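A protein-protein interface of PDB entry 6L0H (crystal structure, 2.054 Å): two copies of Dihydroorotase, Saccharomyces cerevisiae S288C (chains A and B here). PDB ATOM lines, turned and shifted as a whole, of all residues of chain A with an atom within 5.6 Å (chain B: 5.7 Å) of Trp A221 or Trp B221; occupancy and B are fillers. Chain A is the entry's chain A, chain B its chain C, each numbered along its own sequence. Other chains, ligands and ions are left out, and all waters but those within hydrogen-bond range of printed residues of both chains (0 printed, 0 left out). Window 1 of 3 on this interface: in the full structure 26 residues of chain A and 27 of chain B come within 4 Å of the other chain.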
ATOM      1  N   VAL A 153      29.770  31.802 -23.552  1.00  0.00           N
ATOM      2  CA  VAL A 153      29.270  32.531 -24.714  1.00  0.00           C
ATOM      3  C   VAL A 153      28.396  33.706 -24.329  1.00  0.00           C
ATOM      4  O   VAL A 153      28.226  34.623 -25.138  1.00  0.00           O
ATOM      5  CB  VAL A 153      28.507  31.627 -25.713  1.00  0.00           C
ATOM      6  CG1 VAL A 153      29.475  30.693 -26.432  1.00  0.00           C
ATOM      7  CG2 VAL A 153      27.401  30.865 -25.028  1.00  0.00           C
ATOM      8  N   LEU A 154      27.815  33.704 -23.125  1.00  0.00           N
ATOM      9  CA  LEU A 154      26.938  34.813 -22.734  1.00  0.00           C
ATOM     10  C   LEU A 154      27.683  36.032 -22.198  1.00  0.00           C
ATOM     11  O   LEU A 154      27.218  37.156 -22.395  1.00  0.00           O
ATOM     12  CB  LEU A 154      25.922  34.363 -21.696  1.00  0.00           C
ATOM     13  CG  LEU A 154      24.849  33.418 -22.197  1.00  0.00           C
ATOM     14  CD1 LEU A 154      23.863  33.368 -21.097  1.00  0.00           C
ATOM     15  CD2 LEU A 154      24.195  33.880 -23.498  1.00  0.00           C
ATOM     16  N   LEU A 216      16.490  39.091 -32.360  1.00  0.00           N
ATOM     17  CA  LEU A 216      16.704  37.777 -31.768  1.00  0.00           C
ATOM     18  C   LEU A 216      17.058  37.873 -30.301  1.00  0.00           C
ATOM     19  O   LEU A 216      17.672  38.841 -29.830  1.00  0.00           O
ATOM     20  CB  LEU A 216      17.824  37.003 -32.463  1.00  0.00           C
ATOM     21  CG  LEU A 216      17.611  36.703 -33.935  1.00  0.00           C
ATOM     22  CD1 LEU A 216      18.833  35.979 -34.493  1.00  0.00           C
ATOM     23  CD2 LEU A 216      16.316  35.916 -34.171  1.00  0.00           C
ATOM     24  N   THR A 217      16.694  36.806 -29.609  1.00  0.00           N
ATOM     25  CA  THR A 217      16.977  36.532 -28.221  1.00  0.00           C
ATOM     26  C   THR A 217      17.439  35.070 -28.141  1.00  0.00           C
ATOM     27  O   THR A 217      17.324  34.310 -29.116  1.00  0.00           O
ATOM     28  CB  THR A 217      15.698  36.852 -27.418  1.00  0.00           C
ATOM     29  OG1 THR A 217      15.864  38.100 -26.738  1.00  0.00           O
ATOM     30  CG2 THR A 217      15.295  35.774 -26.491  1.00  0.00           C
ATOM     31  N   ILE A 218      17.998  34.679 -26.989  1.00  0.00           N
ATOM     32  CA  ILE A 218      18.489  33.312 -26.818  1.00  0.00           C
ATOM     33  C   ILE A 218      17.419  32.289 -27.178  1.00  0.00           C
ATOM     34  O   ILE A 218      17.725  31.249 -27.774  1.00  0.00           O
ATOM     35  CB  ILE A 218      19.022  33.082 -25.385  1.00  0.00           C
ATOM     36  CG1 ILE A 218      19.546  31.648 -25.260  1.00  0.00           C
ATOM     37  CG2 ILE A 218      17.942  33.361 -24.324  1.00  0.00           C
ATOM     38  CD1 ILE A 218      20.432  31.422 -24.055  1.00  0.00           C
ATOM     39  N   ASP A 219      16.153  32.571 -26.852  1.00  0.00           N
ATOM     40  CA  ASP A 219      15.072  31.657 -27.220  1.00  0.00           C
ATOM     41  C   ASP A 219      14.979  31.421 -28.721  1.00  0.00           C
ATOM     42  O   ASP A 219      14.556  30.342 -29.144  1.00  0.00           O
ATOM     43  CB  ASP A 219      13.734  32.164 -26.703  1.00  0.00           C
ATOM     44  CG  ASP A 219      13.448  31.700 -25.290  1.00  0.00           C
ATOM     45  OD1 ASP A 219      14.413  31.338 -24.592  1.00  0.00           O
ATOM     46  OD2 ASP A 219      12.267  31.712 -24.882  1.00  0.00           O
ATOM     47  N   ASP A 220      15.329  32.410 -29.541  1.00  0.00           N
ATOM     48  CA  ASP A 220      15.178  32.222 -30.973  1.00  0.00           C
ATOM     49  C   ASP A 220      16.207  31.266 -31.555  1.00  0.00           C
ATOM     50  O   ASP A 220      15.935  30.652 -32.594  1.00  0.00           O
ATOM     51  CB  ASP A 220      15.266  33.563 -31.700  1.00  0.00           C
ATOM     52  CG  ASP A 220      14.215  34.536 -31.253  1.00  0.00           C
ATOM     53  OD1 ASP A 220      13.017  34.218 -31.379  1.00  0.00           O
ATOM     54  OD2 ASP A 220      14.587  35.622 -30.766  1.00  0.00           O
ATOM     55  N   TRP A 221      17.377  31.091 -30.929  1.00  0.00           N
ATOM     56  CA  TRP A 221      18.338  30.150 -31.490  1.00  0.00           C
ATOM     57  C   TRP A 221      18.499  28.872 -30.668  1.00  0.00           C
ATOM     58  O   TRP A 221      19.220  27.964 -31.111  1.00  0.00           O
ATOM     59  CB  TRP A 221      19.714  30.810 -31.700  1.00  0.00           C
ATOM     60  CG  TRP A 221      20.380  31.405 -30.474  1.00  0.00           C
ATOM     61  CD1 TRP A 221      20.261  32.692 -30.010  1.00  0.00           C
ATOM     62  CD2 TRP A 221      21.303  30.748 -29.590  1.00  0.00           C
ATOM     63  NE1 TRP A 221      21.041  32.868 -28.888  1.00  0.00           N
ATOM     64  CE2 TRP A 221      21.681  31.686 -28.605  1.00  0.00           C
ATOM     65  CE3 TRP A 221      21.835  29.449 -29.528  1.00  0.00           C
ATOM     66  CZ2 TRP A 221      22.561  31.366 -27.571  1.00  0.00           C
ATOM     67  CZ3 TRP A 221      22.708  29.134 -28.507  1.00  0.00           C
ATOM     68  CH2 TRP A 221      23.069  30.089 -27.541  1.00  0.00           C
ATOM     69  N   ALA A 222      17.909  28.804 -29.470  1.00  0.00           N
ATOM     70  CA  ALA A 222      17.888  27.584 -28.665  1.00  0.00           C
ATOM     71  C   ALA A 222      17.089  26.535 -29.421  1.00  0.00           C
ATOM     72  O   ALA A 222      15.858  26.513 -29.348  1.00  0.00           O
ATOM     73  CB  ALA A 222      17.292  27.848 -27.283  1.00  0.00           C
ATOM     74  N   GLY A 223      17.771  25.679 -30.156  1.00  0.00           N
ATOM     75  CA  GLY A 223      17.117  24.691 -30.982  1.00  0.00           C
ATOM     76  C   GLY A 223      16.955  25.102 -32.434  1.00  0.00           C
ATOM     77  O   GLY A 223      16.443  24.301 -33.228  1.00  0.00           O
ATOM     78  N   ASN A 224      17.433  26.292 -32.831  1.00  0.00           N
ATOM     79  CA  ASN A 224      17.342  26.742 -34.225  1.00  0.00           C
ATOM     80  C   ASN A 224      18.716  27.201 -34.679  1.00  0.00           C
ATOM     81  O   ASN A 224      19.025  28.402 -34.659  1.00  0.00           O
ATOM     82  CB  ASN A 224      16.314  27.855 -34.408  1.00  0.00           C
ATOM     83  CG  ASN A 224      14.932  27.447 -33.952  1.00  0.00           C
ATOM     84  OD1 ASN A 224      14.412  26.408 -34.362  1.00  0.00           O
ATOM     85  ND2 ASN A 224      14.323  28.267 -33.098  1.00  0.00           N
ATOM     86  N   PRO A 225      19.554  26.275 -35.121  1.00  0.00           N
ATOM     87  CA  PRO A 225      20.872  26.666 -35.632  1.00  0.00           C
ATOM     88  C   PRO A 225      20.824  27.751 -36.688  1.00  0.00           C
ATOM     89  O   PRO A 225      21.808  28.484 -36.819  1.00  0.00           O
ATOM     90  CB  PRO A 225      21.426  25.349 -36.190  1.00  0.00           C
ATOM     91  CG  PRO A 225      20.793  24.307 -35.324  1.00  0.00           C
ATOM     92  CD  PRO A 225      19.411  24.808 -35.018  1.00  0.00           C
ATOM     93  N   ASN A 227      19.389  30.465 -36.540  1.00  0.00           N
ATOM     94  CA  ASN A 227      19.532  31.730 -35.842  1.00  0.00           C
ATOM     95  C   ASN A 227      20.782  31.788 -34.981  1.00  0.00           C
ATOM     96  O   ASN A 227      20.950  32.745 -34.212  1.00  0.00           O
ATOM     97  CB  ASN A 227      18.303  32.001 -34.998  1.00  0.00           C
ATOM     98  CG  ASN A 227      17.113  32.353 -35.840  1.00  0.00           C
ATOM     99  OD1 ASN A 227      17.250  33.026 -36.868  1.00  0.00           O
ATOM    100  ND2 ASN A 227      15.928  31.901 -35.418  1.00  0.00           N
ATOM    101  N   PHE A 228      21.662  30.791 -35.091  1.00  0.00           N
ATOM    102  CA  PHE A 228      22.868  30.735 -34.276  1.00  0.00           C
ATOM    103  C   PHE A 228      23.971  31.529 -34.956  1.00  0.00           C
ATOM    104  O   PHE A 228      24.316  31.252 -36.108  1.00  0.00           O
ATOM    105  CB  PHE A 228      23.310  29.290 -34.063  1.00  0.00           C
ATOM    106  CG  PHE A 228      24.674  29.160 -33.466  1.00  0.00           C
ATOM    107  CD1 PHE A 228      24.937  29.659 -32.212  1.00  0.00           C
ATOM    108  CD2 PHE A 228      25.685  28.515 -34.156  1.00  0.00           C
ATOM    109  CE1 PHE A 228      26.220  29.526 -31.636  1.00  0.00           C
ATOM    110  CE2 PHE A 228      26.962  28.385 -33.609  1.00  0.00           C
ATOM    111  CZ  PHE A 228      27.225  28.897 -32.338  1.00  0.00           C
ATOM    112  N   VAL A 232      26.632  35.421 -29.722  1.00  0.00           N
ATOM    113  CA  VAL A 232      25.314  34.821 -29.619  1.00  0.00           C
ATOM    114  C   VAL A 232      24.286  35.889 -29.214  1.00  0.00           C
ATOM    115  O   VAL A 232      24.592  36.803 -28.441  1.00  0.00           O
ATOM    116  CB  VAL A 232      25.473  33.680 -28.596  1.00  0.00           C
ATOM    117  CG1 VAL A 232      24.695  33.902 -27.330  1.00  0.00           C
ATOM    118  CG2 VAL A 232      25.346  32.323 -29.221  1.00  0.00           C
ATOM    119  N   ALA A 233      23.065  35.802 -29.758  1.00  0.00           N
ATOM    120  CA  ALA A 233      21.974  36.636 -29.244  1.00  0.00           C
ATOM    121  C   ALA A 233      21.683  36.301 -27.782  1.00  0.00           C
ATOM    122  O   ALA A 233      21.612  35.130 -27.399  1.00  0.00           O
ATOM    123  CB  ALA A 233      20.696  36.457 -30.081  1.00  0.00           C
ATOM    124  N   LYS A 234      21.492  37.330 -26.967  1.00  0.00           N
ATOM    125  CA  LYS A 234      21.502  37.186 -25.512  1.00  0.00           C
ATOM    126  C   LYS A 234      20.093  37.420 -24.969  1.00  0.00           C
ATOM    127  O   LYS A 234      19.149  36.832 -25.506  1.00  0.00           O
ATOM    128  CB  LYS A 234      22.602  38.076 -24.949  1.00  0.00           C
ATOM    129  CG  LYS A 234      23.976  37.712 -25.559  1.00  0.00           C
ATOM    130  CD  LYS A 234      25.108  38.576 -25.061  1.00  0.00           C
ATOM    131  CE  LYS A 234      26.463  37.982 -25.465  1.00  0.00           C
ATOM    132  NZ  LYS A 234      26.606  37.759 -26.945  1.00  0.00           N
ATOM    133  N   VAL B 153      14.715  30.418 -22.051  1.00  0.00           N
ATOM    134  CA  VAL B 153      15.277  29.121 -21.699  1.00  0.00           C
ATOM    135  C   VAL B 153      16.266  29.240 -20.536  1.00  0.00           C
ATOM    136  O   VAL B 153      16.482  28.271 -19.809  1.00  0.00           O
ATOM    137  CB  VAL B 153      15.914  28.448 -22.937  1.00  0.00           C
ATOM    138  CG1 VAL B 153      14.852  28.121 -23.986  1.00  0.00           C
ATOM    139  CG2 VAL B 153      17.002  29.319 -23.535  1.00  0.00           C
ATOM    140  N   LEU B 216      27.876  19.382 -18.946  1.00  0.00           N
ATOM    141  CA  LEU B 216      27.588  20.340 -19.999  1.00  0.00           C
ATOM    142  C   LEU B 216      27.423  21.743 -19.446  1.00  0.00           C
ATOM    143  O   LEU B 216      27.041  21.944 -18.287  1.00  0.00           O
ATOM    144  CB  LEU B 216      26.322  19.965 -20.771  1.00  0.00           C
ATOM    145  CG  LEU B 216      26.344  18.772 -21.721  1.00  0.00           C
ATOM    146  CD1 LEU B 216      24.984  18.655 -22.420  1.00  0.00           C
ATOM    147  CD2 LEU B 216      27.501  18.825 -22.738  1.00  0.00           C
ATOM    148  N   THR B 217      27.727  22.707 -20.308  1.00  0.00           N
ATOM    149  CA  THR B 217      27.521  24.130 -20.095  1.00  0.00           C
ATOM    150  C   THR B 217      26.900  24.685 -21.375  1.00  0.00           C
ATOM    151  O   THR B 217      26.904  24.014 -22.409  1.00  0.00           O
ATOM    152  CB  THR B 217      28.893  24.768 -19.737  1.00  0.00           C
ATOM    153  OG1 THR B 217      28.956  25.099 -18.343  1.00  0.00           O
ATOM    154  CG2 THR B 217      29.259  25.933 -20.587  1.00  0.00           C
ATOM    155  N   ILE B 218      26.344  25.903 -21.325  1.00  0.00           N
ATOM    156  CA  ILE B 218      25.780  26.487 -22.551  1.00  0.00           C
ATOM    157  C   ILE B 218      26.787  26.465 -23.705  1.00  0.00           C
ATOM    158  O   ILE B 218      26.401  26.312 -24.871  1.00  0.00           O
ATOM    159  CB  ILE B 218      25.258  27.912 -22.298  1.00  0.00           C
ATOM    160  CG1 ILE B 218      24.614  28.472 -23.574  1.00  0.00           C
ATOM    161  CG2 ILE B 218      26.374  28.832 -21.811  1.00  0.00           C
ATOM    162  CD1 ILE B 218      23.903  29.792 -23.370  1.00  0.00           C
ATOM    163  N   ASP B 219      28.082  26.627 -23.409  1.00  0.00           N
ATOM    164  CA  ASP B 219      29.117  26.549 -24.443  1.00  0.00           C
ATOM    165  C   ASP B 219      29.089  25.233 -25.204  1.00  0.00           C
ATOM    166  O   ASP B 219      29.413  25.202 -26.395  1.00  0.00           O
ATOM    167  CB  ASP B 219      30.501  26.709 -23.819  1.00  0.00           C
ATOM    168  CG  ASP B 219      30.824  28.124 -23.499  1.00  0.00           C
ATOM    169  OD1 ASP B 219      29.879  28.928 -23.385  1.00  0.00           O
ATOM    170  OD2 ASP B 219      32.022  28.423 -23.344  1.00  0.00           O
ATOM    171  N   ASP B 220      28.747  24.134 -24.538  1.00  0.00           N
ATOM    172  CA  ASP B 220      28.795  22.829 -25.184  1.00  0.00           C
ATOM    173  C   ASP B 220      27.640  22.564 -26.144  1.00  0.00           C
ATOM    174  O   ASP B 220      27.782  21.714 -27.035  1.00  0.00           O
ATOM    175  CB  ASP B 220      28.869  21.740 -24.110  1.00  0.00           C
ATOM    176  CG  ASP B 220      30.048  21.945 -23.155  1.00  0.00           C
ATOM    177  OD1 ASP B 220      31.171  22.130 -23.656  1.00  0.00           O
ATOM    178  OD2 ASP B 220      29.857  21.951 -21.916  1.00  0.00           O
ATOM    179  N   TRP B 221      26.495  23.232 -25.998  1.00  0.00           N
ATOM    180  CA  TRP B 221      25.399  22.998 -26.931  1.00  0.00           C
ATOM    181  C   TRP B 221      25.129  24.170 -27.876  1.00  0.00           C
ATOM    182  O   TRP B 221      24.324  24.016 -28.798  1.00  0.00           O
ATOM    183  CB  TRP B 221      24.097  22.609 -26.195  1.00  0.00           C
ATOM    184  CG  TRP B 221      23.506  23.639 -25.259  1.00  0.00           C
ATOM    185  CD1 TRP B 221      23.662  23.696 -23.907  1.00  0.00           C
ATOM    186  CD2 TRP B 221      22.655  24.735 -25.610  1.00  0.00           C
ATOM    187  NE1 TRP B 221      22.982  24.775 -23.387  1.00  0.00           N
ATOM    188  CE2 TRP B 221      22.338  25.419 -24.411  1.00  0.00           C
ATOM    189  CE3 TRP B 221      22.117  25.198 -26.818  1.00  0.00           C
ATOM    190  CZ2 TRP B 221      21.528  26.545 -24.388  1.00  0.00           C
ATOM    191  CZ3 TRP B 221      21.313  26.307 -26.796  1.00  0.00           C
ATOM    192  CH2 TRP B 221      21.026  26.981 -25.587  1.00  0.00           C
ATOM    193  N   ALA B 222      25.825  25.302 -27.730  1.00  0.00           N
ATOM    194  CA  ALA B 222      25.520  26.468 -28.572  1.00  0.00           C
ATOM    195  C   ALA B 222      25.625  26.139 -30.063  1.00  0.00           C
ATOM    196  O   ALA B 222      24.722  26.449 -30.853  1.00  0.00           O
ATOM    197  CB  ALA B 222      26.439  27.635 -28.194  1.00  0.00           C
ATOM    198  N   GLY B 223      26.715  25.501 -30.471  1.00  0.00           N
ATOM    199  CA  GLY B 223      26.867  25.062 -31.844  1.00  0.00           C
ATOM    200  C   GLY B 223      26.723  23.571 -32.042  1.00  0.00           C
ATOM    201  O   GLY B 223      27.036  23.073 -33.132  1.00  0.00           O
ATOM    202  N   ASN B 224      26.288  22.825 -31.027  1.00  0.00           N
ATOM    203  CA  ASN B 224      26.215  21.363 -31.079  1.00  0.00           C
ATOM    204  C   ASN B 224      24.830  20.872 -30.687  1.00  0.00           C
ATOM    205  O   ASN B 224      24.582  20.598 -29.504  1.00  0.00           O
ATOM    206  CB  ASN B 224      27.254  20.735 -30.154  1.00  0.00           C
ATOM    207  CG  ASN B 224      28.674  21.092 -30.536  1.00  0.00           C
ATOM    208  OD1 ASN B 224      29.084  20.919 -31.686  1.00  0.00           O
ATOM    209  ND2 ASN B 224      29.445  21.563 -29.560  1.00  0.00           N
ATOM    210  N   PRO B 225      23.901  20.767 -31.648  1.00  0.00           N
ATOM    211  CA  PRO B 225      22.548  20.264 -31.341  1.00  0.00           C
ATOM    212  C   PRO B 225      22.506  18.930 -30.610  1.00  0.00           C
ATOM    213  O   PRO B 225      21.533  18.657 -29.896  1.00  0.00           O
ATOM    214  CB  PRO B 225      21.917  20.122 -32.732  1.00  0.00           C
ATOM    215  CG  PRO B 225      22.661  21.116 -33.578  1.00  0.00           C
ATOM    216  CD  PRO B 225      24.065  21.068 -33.078  1.00  0.00           C
ATOM    217  N   ASN B 227      24.079  18.158 -28.123  1.00  0.00           N
ATOM    218  CA  ASN B 227      24.099  18.468 -26.694  1.00  0.00           C
ATOM    219  C   ASN B 227      22.928  19.343 -26.241  1.00  0.00           C
ATOM    220  O   ASN B 227      22.916  19.802 -25.092  1.00  0.00           O
ATOM    221  CB  ASN B 227      25.413  19.147 -26.317  1.00  0.00           C
ATOM    222  CG  ASN B 227      26.565  18.186 -26.301  1.00  0.00           C
ATOM    223  OD1 ASN B 227      26.375  16.972 -26.128  1.00  0.00           O
ATOM    224  ND2 ASN B 227      27.770  18.708 -26.487  1.00  0.00           N
ATOM    225  N   PHE B 228      21.959  19.593 -27.114  1.00  0.00           N
ATOM    226  CA  PHE B 228      20.817  20.442 -26.794  1.00  0.00           C
ATOM    227  C   PHE B 228      19.744  19.600 -26.125  1.00  0.00           C
ATOM    228  O   PHE B 228      19.354  18.555 -26.654  1.00  0.00           O
ATOM    229  CB  PHE B 228      20.262  21.106 -28.061  1.00  0.00           C
ATOM    230  CG  PHE B 228      18.977  21.868 -27.843  1.00  0.00           C
ATOM    231  CD1 PHE B 228      18.930  22.973 -27.002  1.00  0.00           C
ATOM    232  CD2 PHE B 228      17.812  21.488 -28.493  1.00  0.00           C
ATOM    233  CE1 PHE B 228      17.751  23.678 -26.810  1.00  0.00           C
ATOM    234  CE2 PHE B 228      16.616  22.197 -28.291  1.00  0.00           C
ATOM    235  CZ  PHE B 228      16.595  23.295 -27.446  1.00  0.00           C
ATOM    236  N   CYS B 229      19.290  20.039 -24.956  1.00  0.00           N
ATOM    237  CA  CYS B 229      18.257  19.327 -24.222  1.00  0.00           C
ATOM    238  C   CYS B 229      17.450  20.341 -23.430  1.00  0.00           C
ATOM    239  O   CYS B 229      17.830  21.513 -23.318  1.00  0.00           O
ATOM    240  CB  CYS B 229      18.856  18.267 -23.286  1.00  0.00           C
ATOM    241  SG  CYS B 229      19.778  18.984 -21.883  1.00  0.00           S
ATOM    242  N   VAL B 232      17.884  23.567 -20.685  1.00  0.00           N
ATOM    243  CA  VAL B 232      19.196  23.697 -21.305  1.00  0.00           C
ATOM    244  C   VAL B 232      20.266  23.708 -20.227  1.00  0.00           C
ATOM    245  O   VAL B 232      20.036  24.168 -19.098  1.00  0.00           O
ATOM    246  CB  VAL B 232      19.289  24.966 -22.176  1.00  0.00           C
ATOM    247  CG1 VAL B 232      18.254  24.930 -23.322  1.00  0.00           C
ATOM    248  CG2 VAL B 232      19.150  26.235 -21.325  1.00  0.00           C
ATOM    249  N   ALA B 233      21.435  23.163 -20.564  1.00  0.00           N
ATOM    250  CA  ALA B 233      22.616  23.373 -19.732  1.00  0.00           C
ATOM    251  C   ALA B 233      22.957  24.864 -19.668  1.00  0.00           C
ATOM    252  O   ALA B 233      22.940  25.568 -20.684  1.00  0.00           O
ATOM    253  CB  ALA B 233      23.798  22.585 -20.289  1.00  0.00           C
ATOM    254  N   LYS B 234      23.285  25.345 -18.477  1.00  0.00           N
ATOM    255  CA  LYS B 234      23.357  26.776 -18.198  1.00  0.00           C
ATOM    256  C   LYS B 234      24.811  27.176 -17.952  1.00  0.00           C
ATOM    257  O   LYS B 234      25.679  26.743 -18.715  1.00  0.00           O
ATOM    258  CB  LYS B 234      22.387  27.100 -17.075  1.00  0.00           C
ATOM    259  CG  LYS B 234      20.926  26.971 -17.532  1.00  0.00           C
ATOM    260  CD  LYS B 234      19.949  27.028 -16.361  1.00  0.00           C
ATOM    261  CE  LYS B 234      18.498  26.951 -16.866  1.00  0.00           C
ATOM    262  NZ  LYS B 234      18.123  25.620 -17.465  1.00  0.00           N
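OD1 of Asp B219 lies within hydrogen-bond range of N of Val A153 (2.9 Å).
The side-chain carboxylate of Asp A219 lies within hydrogen-bond range of the backbone NH of Val B153, at 2.7 Å.
The backbone carbonyl oxygen of Lys A234 lies within hydrogen-bond range of the backbone NH of Ile A218 (2.9 Å).
The backbone carbonyl oxygen (O) of Ala A233 lies within hydrogen-bond range of the indole nitrogen (NE1) of Trp A221 (2.8 Å).
The backbone NH of Ile B218 lies within hydrogen-bond range of the backbone carbonyl oxygen of Ala B233, at 3.5 Å.
The backbone carbonyl oxygen of Lys B234 sits at hydrogen-bond distance from the backbone NH of Ile B218, 2.8 Å away.
NE1 of Trp B221 lies within hydrogen-bond range of O of Ala B233 (2.8 Å).
CG2 of Val A153 touches CG2 of Ile B218, at 3.9 Å.
Leu A154 touches Ile B218.
Ile A218 touches Val B153.
Ile B218 touches Ile A218.
Trp A221 touches Trp B221.
CZ3 of Trp A221 touches CA of Ala B222 (3.9 Å).
Ala A222 touches Phe B228.
Phe B228 touches Gly A223 (CE2 to CA, 3.7 Å).
Ala B222 touches Phe A228.
Phe A228 touches Gly B223.
Trp A221 touches two residues of chain B.
Printed residues of chain A within 4 Å of Ile B218: Val A153, Leu A154 and Ile A218.
Of the printed residues of chain A, Trp B221 touches Trp A221.
Printed residues of chain A within 4 Å of Ala B222: Trp A221 (3.9 Å) and Phe A228 (3.5 Å).
Of the printed residues of chain A, Phe B228 touches Ala A222 and Gly A223.
The nearest printed residue of chain B that does not touch Val A153 is Ala B222 (4.6 Å).
Of the 17 printed residues of chain A, 8 touch a printed residue of chain B.
Hydrophobic or aromatic side chains of chain A that line the printed part of chain B: Val A153, Leu A154, Ile A218, Trp A221 and Phe A228.
Among the printed residues, 12 pairs touch across the chains.
Val A153 touches Asp B219, and with the chains exchanged Asp A219 touches Val B153.
Ile B218 touches its own counterpart, Ile A218.
Trp A221 touches its own counterpart, Trp B221.
Gly A223 touches Phe B228, and with the chains exchanged Phe A228 touches Gly B223.
16 positions are printed for both chains.
Of the 12 pairs that touch across the chains among the printed residues, 10 have their exchanged pair printed and touching as well.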
